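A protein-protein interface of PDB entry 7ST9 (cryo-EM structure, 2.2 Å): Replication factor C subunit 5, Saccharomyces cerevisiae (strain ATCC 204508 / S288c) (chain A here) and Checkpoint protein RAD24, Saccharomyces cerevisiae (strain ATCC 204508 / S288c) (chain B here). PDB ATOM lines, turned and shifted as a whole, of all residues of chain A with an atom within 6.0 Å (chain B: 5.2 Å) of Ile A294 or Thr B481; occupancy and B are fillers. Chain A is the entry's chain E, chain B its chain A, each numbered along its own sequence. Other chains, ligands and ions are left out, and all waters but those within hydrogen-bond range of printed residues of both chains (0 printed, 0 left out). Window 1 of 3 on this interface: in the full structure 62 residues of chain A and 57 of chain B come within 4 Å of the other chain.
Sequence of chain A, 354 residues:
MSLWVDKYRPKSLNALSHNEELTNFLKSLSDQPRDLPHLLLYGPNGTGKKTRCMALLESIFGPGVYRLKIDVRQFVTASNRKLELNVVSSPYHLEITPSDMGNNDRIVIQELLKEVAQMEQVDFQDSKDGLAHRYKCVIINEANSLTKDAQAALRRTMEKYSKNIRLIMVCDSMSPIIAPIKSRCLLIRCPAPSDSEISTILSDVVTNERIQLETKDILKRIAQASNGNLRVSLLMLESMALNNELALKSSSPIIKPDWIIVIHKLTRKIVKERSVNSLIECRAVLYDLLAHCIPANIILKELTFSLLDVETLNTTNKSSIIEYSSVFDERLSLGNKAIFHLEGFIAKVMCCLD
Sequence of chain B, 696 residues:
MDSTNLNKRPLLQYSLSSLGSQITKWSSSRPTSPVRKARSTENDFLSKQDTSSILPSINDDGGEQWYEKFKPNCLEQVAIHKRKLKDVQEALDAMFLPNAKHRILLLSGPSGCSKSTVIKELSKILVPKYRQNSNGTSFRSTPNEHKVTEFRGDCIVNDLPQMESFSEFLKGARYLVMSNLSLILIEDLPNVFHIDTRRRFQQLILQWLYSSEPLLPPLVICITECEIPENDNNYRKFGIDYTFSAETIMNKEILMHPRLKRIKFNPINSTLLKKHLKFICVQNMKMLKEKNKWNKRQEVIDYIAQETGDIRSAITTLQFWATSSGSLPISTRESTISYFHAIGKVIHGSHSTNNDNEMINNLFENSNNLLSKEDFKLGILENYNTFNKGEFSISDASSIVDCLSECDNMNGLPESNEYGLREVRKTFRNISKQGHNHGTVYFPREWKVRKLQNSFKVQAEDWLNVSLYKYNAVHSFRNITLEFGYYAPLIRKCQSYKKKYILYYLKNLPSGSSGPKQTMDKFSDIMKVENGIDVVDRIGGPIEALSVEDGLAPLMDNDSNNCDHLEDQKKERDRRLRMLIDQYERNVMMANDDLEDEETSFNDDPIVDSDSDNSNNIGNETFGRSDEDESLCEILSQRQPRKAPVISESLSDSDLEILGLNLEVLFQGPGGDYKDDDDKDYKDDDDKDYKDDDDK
The backbone carbonyl oxygen of Leu B482 sits at hydrogen-bond distance from the indole nitrogen of Trp A259 (3.1 Å).
The backbone carbonyl oxygen of Arg B478 is in hydrogen-bond range of the side-chain hydroxyl of Thr B481 (2.5 Å). The backbone carbonyl oxygen (O) of Phe B477 sits close to the side-chain hydroxyl (OG1) of Thr B481, 3.5 Å away.
Among the printed residues, pairs that only touch across the chains: Ile A294 with Thr B481 (3.1 Å), His A292 with Arg B538 (3.4 Å), Ile A298 with Arg B478 (3.5 Å), His A292 with Phe B456 (3.5 Å), Cys A293 with Phe B456 (3.6 Å) and Cys A293 with Thr B481 (3.7 Å).
Of the printed residues of chain B, His A292 touches Phe B456 and Arg B538. Printed residues of chain B within 4 Å of Cys A293: Phe B456 (3.6 Å) and Thr B481 (3.7 Å). Pro A295 touches none of the printed residues of chain B. Of the printed residues of chain B, Ile A298 touches Arg B478 (3.5 Å). Of chain A, only Cys A293 (3.7 Å) and Ile A294 (3.1 Å) come within 4 Å of Thr B481. The nearest residue of chain B that does not touch Ile A294 is Leu B482 (4.6 Å). The nearest residue of chain A that does not touch Thr B481 is His A292 (4.3 Å). The nearest printed residue of chain A that does not touch Leu B482 is Ile A298 (4.2 Å).
Among the printed residues, no Asp or Glu carboxylate lies within 4 Å of a Lys or Arg side-chain nitrogen of the other chain.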
ATOM      1  N   TRP A 259       0.652 -14.334 -23.874  1.00  0.00           N
ATOM      2  CA  TRP A 259       0.483 -15.108 -22.650  1.00  0.00           C
ATOM      3  C   TRP A 259      -0.386 -14.370 -21.638  1.00  0.00           C
ATOM      4  O   TRP A 259      -1.072 -15.007 -20.831  1.00  0.00           O
ATOM      5  CB  TRP A 259       1.849 -15.454 -22.050  1.00  0.00           C
ATOM      6  CG  TRP A 259       2.669 -14.272 -21.632  1.00  0.00           C
ATOM      7  CD1 TRP A 259       3.365 -13.426 -22.446  1.00  0.00           C
ATOM      8  CD2 TRP A 259       2.895 -13.816 -20.293  1.00  0.00           C
ATOM      9  NE1 TRP A 259       4.004 -12.467 -21.698  1.00  0.00           N
ATOM     10  CE2 TRP A 259       3.732 -12.685 -20.374  1.00  0.00           C
ATOM     11  CE3 TRP A 259       2.469 -14.251 -19.035  1.00  0.00           C
ATOM     12  CZ2 TRP A 259       4.149 -11.983 -19.245  1.00  0.00           C
ATOM     13  CZ3 TRP A 259       2.883 -13.555 -17.917  1.00  0.00           C
ATOM     14  CH2 TRP A 259       3.714 -12.433 -18.028  1.00  0.00           C
ATOM     15  N   LEU A 289       1.623 -22.802 -21.138  1.00  0.00           N
ATOM     16  CA  LEU A 289       2.368 -21.604 -20.761  1.00  0.00           C
ATOM     17  C   LEU A 289       3.806 -21.942 -20.390  1.00  0.00           C
ATOM     18  O   LEU A 289       4.742 -21.239 -20.788  1.00  0.00           O
ATOM     19  CB  LEU A 289       1.673 -20.897 -19.597  1.00  0.00           C
ATOM     20  CG  LEU A 289       0.396 -20.131 -19.942  1.00  0.00           C
ATOM     21  CD1 LEU A 289      -0.363 -19.770 -18.677  1.00  0.00           C
ATOM     22  CD2 LEU A 289       0.718 -18.884 -20.755  1.00  0.00           C
ATOM     23  N   LEU A 290       4.002 -23.018 -19.624  1.00  0.00           N
ATOM     24  CA  LEU A 290       5.348 -23.403 -19.214  1.00  0.00           C
ATOM     25  C   LEU A 290       6.184 -23.874 -20.397  1.00  0.00           C
ATOM     26  O   LEU A 290       7.415 -23.762 -20.367  1.00  0.00           O
ATOM     27  CB  LEU A 290       5.281 -24.497 -18.148  1.00  0.00           C
ATOM     28  CG  LEU A 290       4.760 -24.063 -16.776  1.00  0.00           C
ATOM     29  CD1 LEU A 290       4.373 -25.277 -15.946  1.00  0.00           C
ATOM     30  CD2 LEU A 290       5.793 -23.220 -16.045  1.00  0.00           C
ATOM     31  N   ALA A 291       5.541 -24.405 -21.439  1.00  0.00           N
ATOM     32  CA  ALA A 291       6.284 -24.850 -22.614  1.00  0.00           C
ATOM     33  C   ALA A 291       7.016 -23.696 -23.287  1.00  0.00           C
ATOM     34  O   ALA A 291       8.019 -23.914 -23.974  1.00  0.00           O
ATOM     35  CB  ALA A 291       5.338 -25.526 -23.605  1.00  0.00           C
ATOM     36  N   HIS A 292       6.536 -22.468 -23.103  1.00  0.00           N
ATOM     37  CA  HIS A 292       7.176 -21.286 -23.662  1.00  0.00           C
ATOM     38  C   HIS A 292       8.224 -20.692 -22.727  1.00  0.00           C
ATOM     39  O   HIS A 292       8.671 -19.563 -22.951  1.00  0.00           O
ATOM     40  CB  HIS A 292       6.120 -20.233 -24.006  1.00  0.00           C
ATOM     41  CG  HIS A 292       5.414 -20.492 -25.300  1.00  0.00           C
ATOM     42  ND1 HIS A 292       4.551 -21.552 -25.477  1.00  0.00           N
ATOM     43  CD2 HIS A 292       5.446 -19.833 -26.482  1.00  0.00           C
ATOM     44  CE1 HIS A 292       4.079 -21.533 -26.711  1.00  0.00           C
ATOM     45  NE2 HIS A 292       4.607 -20.500 -27.342  1.00  0.00           N
ATOM     46  N   CYS A 293       8.623 -21.429 -21.689  1.00  0.00           N
ATOM     47  CA  CYS A 293       9.671 -21.001 -20.764  1.00  0.00           C
ATOM     48  C   CYS A 293       9.272 -19.748 -19.989  1.00  0.00           C
ATOM     49  O   CYS A 293      10.126 -18.949 -19.597  1.00  0.00           O
ATOM     50  CB  CYS A 293      10.996 -20.771 -21.496  1.00  0.00           C
ATOM     51  SG  CYS A 293      11.546 -22.178 -22.486  1.00  0.00           S
ATOM     52  N   ILE A 294       7.979 -19.563 -19.761  1.00  0.00           N
ATOM     53  CA  ILE A 294       7.517 -18.496 -18.872  1.00  0.00           C
ATOM     54  C   ILE A 294       7.778 -18.923 -17.429  1.00  0.00           C
ATOM     55  O   ILE A 294       7.391 -20.039 -17.048  1.00  0.00           O
ATOM     56  CB  ILE A 294       6.036 -18.206 -19.099  1.00  0.00           C
ATOM     57  CG1 ILE A 294       5.759 -17.897 -20.576  1.00  0.00           C
ATOM     58  CG2 ILE A 294       5.584 -17.044 -18.222  1.00  0.00           C
ATOM     59  CD1 ILE A 294       6.396 -16.617 -21.083  1.00  0.00           C
ATOM     60  N   PRO A 295       8.425 -18.095 -16.607  1.00  0.00           N
ATOM     61  CA  PRO A 295       8.707 -18.514 -15.228  1.00  0.00           C
ATOM     62  C   PRO A 295       7.428 -18.842 -14.469  1.00  0.00           C
ATOM     63  O   PRO A 295       6.394 -18.196 -14.645  1.00  0.00           O
ATOM     64  CB  PRO A 295       9.425 -17.300 -14.626  1.00  0.00           C
ATOM     65  CG  PRO A 295       9.963 -16.552 -15.787  1.00  0.00           C
ATOM     66  CD  PRO A 295       8.991 -16.767 -16.902  1.00  0.00           C
ATOM     67  N   ALA A 296       7.513 -19.864 -13.614  1.00  0.00           N
ATOM     68  CA  ALA A 296       6.346 -20.290 -12.848  1.00  0.00           C
ATOM     69  C   ALA A 296       5.872 -19.196 -11.900  1.00  0.00           C
ATOM     70  O   ALA A 296       4.663 -18.974 -11.753  1.00  0.00           O
ATOM     71  CB  ALA A 296       6.669 -21.564 -12.070  1.00  0.00           C
ATOM     72  N   ILE A 298       6.167 -15.967 -12.228  1.00  0.00           N
ATOM     73  CA  ILE A 298       5.493 -14.934 -13.012  1.00  0.00           C
ATOM     74  C   ILE A 298       4.085 -15.383 -13.378  1.00  0.00           C
ATOM     75  O   ILE A 298       3.132 -14.595 -13.325  1.00  0.00           O
ATOM     76  CB  ILE A 298       6.322 -14.589 -14.264  1.00  0.00           C
ATOM     77  CG1 ILE A 298       7.629 -13.891 -13.869  1.00  0.00           C
ATOM     78  CG2 ILE A 298       5.515 -13.715 -15.215  1.00  0.00           C
ATOM     79  CD1 ILE A 298       7.446 -12.495 -13.293  1.00  0.00           C
ATOM     80  N   ILE A 299       3.930 -16.651 -13.768  1.00  0.00           N
ATOM     81  CA  ILE A 299       2.604 -17.172 -14.089  1.00  0.00           C
ATOM     82  C   ILE A 299       1.688 -17.052 -12.880  1.00  0.00           C
ATOM     83  O   ILE A 299       0.539 -16.608 -12.989  1.00  0.00           O
ATOM     84  CB  ILE A 299       2.700 -18.631 -14.572  1.00  0.00           C
ATOM     85  CG1 ILE A 299       3.422 -18.707 -15.917  1.00  0.00           C
ATOM     86  CG2 ILE A 299       1.309 -19.246 -14.678  1.00  0.00           C
ATOM     87  CD1 ILE A 299       3.923 -20.094 -16.267  1.00  0.00           C
ATOM     88  N   PHE B 456      12.466 -23.985 -27.601  1.00  0.00           N
ATOM     89  CA  PHE B 456      12.319 -22.551 -27.382  1.00  0.00           C
ATOM     90  C   PHE B 456      13.660 -21.910 -27.059  1.00  0.00           C
ATOM     91  O   PHE B 456      13.952 -20.806 -27.526  1.00  0.00           O
ATOM     92  CB  PHE B 456      11.321 -22.291 -26.252  1.00  0.00           C
ATOM     93  CG  PHE B 456      11.024 -20.833 -26.028  1.00  0.00           C
ATOM     94  CD1 PHE B 456      11.917 -20.023 -25.343  1.00  0.00           C
ATOM     95  CD2 PHE B 456       9.850 -20.273 -26.498  1.00  0.00           C
ATOM     96  CE1 PHE B 456      11.646 -18.685 -25.140  1.00  0.00           C
ATOM     97  CE2 PHE B 456       9.572 -18.936 -26.295  1.00  0.00           C
ATOM     98  CZ  PHE B 456      10.472 -18.141 -25.614  1.00  0.00           C
ATOM     99  N   PHE B 477      17.611 -13.379 -21.864  1.00  0.00           N
ATOM    100  CA  PHE B 477      16.709 -14.475 -22.196  1.00  0.00           C
ATOM    101  C   PHE B 477      15.351 -14.291 -21.530  1.00  0.00           C
ATOM    102  O   PHE B 477      14.312 -14.627 -22.112  1.00  0.00           O
ATOM    103  CB  PHE B 477      17.335 -15.807 -21.782  1.00  0.00           C
ATOM    104  CG  PHE B 477      16.417 -16.985 -21.934  1.00  0.00           C
ATOM    105  CD1 PHE B 477      16.243 -17.588 -23.167  1.00  0.00           C
ATOM    106  CD2 PHE B 477      15.730 -17.491 -20.843  1.00  0.00           C
ATOM    107  CE1 PHE B 477      15.400 -18.672 -23.311  1.00  0.00           C
ATOM    108  CE2 PHE B 477      14.886 -18.576 -20.980  1.00  0.00           C
ATOM    109  CZ  PHE B 477      14.720 -19.167 -22.216  1.00  0.00           C
ATOM    110  N   ARG B 478      15.341 -13.766 -20.304  1.00  0.00           N
ATOM    111  CA  ARG B 478      14.083 -13.538 -19.600  1.00  0.00           C
ATOM    112  C   ARG B 478      13.197 -12.566 -20.368  1.00  0.00           C
ATOM    113  O   ARG B 478      11.994 -12.799 -20.535  1.00  0.00           O
ATOM    114  CB  ARG B 478      14.374 -13.011 -18.194  1.00  0.00           C
ATOM    115  CG  ARG B 478      13.196 -13.060 -17.238  1.00  0.00           C
ATOM    116  CD  ARG B 478      13.669 -12.935 -15.797  1.00  0.00           C
ATOM    117  NE  ARG B 478      12.619 -13.240 -14.832  1.00  0.00           N
ATOM    118  CZ  ARG B 478      11.790 -12.346 -14.310  1.00  0.00           C
ATOM    119  NH1 ARG B 478      11.836 -11.070 -14.658  1.00  0.00           N
ATOM    120  NH2 ARG B 478      10.889 -12.743 -13.416  1.00  0.00           N
ATOM    121  N   ASN B 479      13.782 -11.469 -20.854  1.00  0.00           N
ATOM    122  CA  ASN B 479      13.009 -10.506 -21.630  1.00  0.00           C
ATOM    123  C   ASN B 479      12.510 -11.118 -22.931  1.00  0.00           C
ATOM    124  O   ASN B 479      11.420 -10.772 -23.401  1.00  0.00           O
ATOM    125  CB  ASN B 479      13.853  -9.263 -21.913  1.00  0.00           C
ATOM    126  CG  ASN B 479      14.018  -8.380 -20.689  1.00  0.00           C
ATOM    127  OD1 ASN B 479      13.280  -8.509 -19.712  1.00  0.00           O
ATOM    128  ND2 ASN B 479      14.989  -7.478 -20.738  1.00  0.00           N
ATOM    129  N   ILE B 480      13.289 -12.021 -23.529  1.00  0.00           N
ATOM    130  CA  ILE B 480      12.828 -12.712 -24.729  1.00  0.00           C
ATOM    131  C   ILE B 480      11.616 -13.576 -24.410  1.00  0.00           C
ATOM    132  O   ILE B 480      10.624 -13.578 -25.149  1.00  0.00           O
ATOM    133  CB  ILE B 480      13.972 -13.541 -25.344  1.00  0.00           C
ATOM    134  CG1 ILE B 480      15.036 -12.616 -25.938  1.00  0.00           C
ATOM    135  CG2 ILE B 480      13.431 -14.482 -26.412  1.00  0.00           C
ATOM    136  CD1 ILE B 480      16.361 -13.296 -26.204  1.00  0.00           C
ATOM    137  N   THR B 481      11.670 -14.317 -23.300  1.00  0.00           N
ATOM    138  CA  THR B 481      10.534 -15.152 -22.923  1.00  0.00           C
ATOM    139  C   THR B 481       9.308 -14.311 -22.600  1.00  0.00           C
ATOM    140  O   THR B 481       8.178 -14.739 -22.860  1.00  0.00           O
ATOM    141  CB  THR B 481      10.886 -16.036 -21.723  1.00  0.00           C
ATOM    142  OG1 THR B 481      11.239 -15.216 -20.602  1.00  0.00           O
ATOM    143  CG2 THR B 481      12.040 -16.972 -22.052  1.00  0.00           C
ATOM    144  N   LEU B 482       9.504 -13.119 -22.038  1.00  0.00           N
ATOM    145  CA  LEU B 482       8.381 -12.305 -21.592  1.00  0.00           C
ATOM    146  C   LEU B 482       7.847 -11.385 -22.688  1.00  0.00           C
ATOM    147  O   LEU B 482       6.650 -11.417 -22.991  1.00  0.00           O
ATOM    148  CB  LEU B 482       8.788 -11.480 -20.367  1.00  0.00           C
ATOM    149  CG  LEU B 482       9.071 -12.279 -19.090  1.00  0.00           C
ATOM    150  CD1 LEU B 482       9.625 -11.372 -18.004  1.00  0.00           C
ATOM    151  CD2 LEU B 482       7.821 -12.996 -18.602  1.00  0.00           C
ATOM    152  N   GLU B 483       8.706 -10.561 -23.289  1.00  0.00           N
ATOM    153  CA  GLU B 483       8.250  -9.486 -24.165  1.00  0.00           C
ATOM    154  C   GLU B 483       8.721  -9.632 -25.603  1.00  0.00           C
ATOM    155  O   GLU B 483       7.892  -9.628 -26.521  1.00  0.00           O
ATOM    156  CB  GLU B 483       8.716  -8.131 -23.606  1.00  0.00           C
ATOM    157  CG  GLU B 483       8.362  -7.897 -22.143  1.00  0.00           C
ATOM    158  CD  GLU B 483       9.393  -7.052 -21.421  1.00  0.00           C
ATOM    159  OE1 GLU B 483       9.986  -6.159 -22.061  1.00  0.00           O
ATOM    160  OE2 GLU B 483       9.613  -7.282 -20.213  1.00  0.00           O
ATOM    161  N   GLY B 485       9.990 -12.057 -27.460  1.00  0.00           N
ATOM    162  CA  GLY B 485       9.680 -13.251 -28.228  1.00  0.00           C
ATOM    163  C   GLY B 485       8.370 -13.181 -28.982  1.00  0.00           C
ATOM    164  O   GLY B 485       8.196 -13.901 -29.971  1.00  0.00           O
ATOM    165  N   ARG B 538       6.638 -16.111 -34.145  1.00  0.00           N
ATOM    166  CA  ARG B 538       6.636 -16.139 -32.690  1.00  0.00           C
ATOM    167  C   ARG B 538       7.568 -17.232 -32.184  1.00  0.00           C
ATOM    168  O   ARG B 538       7.503 -18.379 -32.633  1.00  0.00           O
ATOM    169  CB  ARG B 538       5.215 -16.373 -32.172  1.00  0.00           C
ATOM    170  CG  ARG B 538       4.905 -15.684 -30.853  1.00  0.00           C
ATOM    171  CD  ARG B 538       5.513 -16.424 -29.674  1.00  0.00           C
ATOM    172  NE  ARG B 538       5.013 -15.927 -28.397  1.00  0.00           N
ATOM    173  CZ  ARG B 538       5.614 -16.113 -27.230  1.00  0.00           C
ATOM    174  NH1 ARG B 538       6.749 -16.787 -27.135  1.00  0.00           N
ATOM    175  NH2 ARG B 538       5.062 -15.612 -26.129  1.00  0.00           N
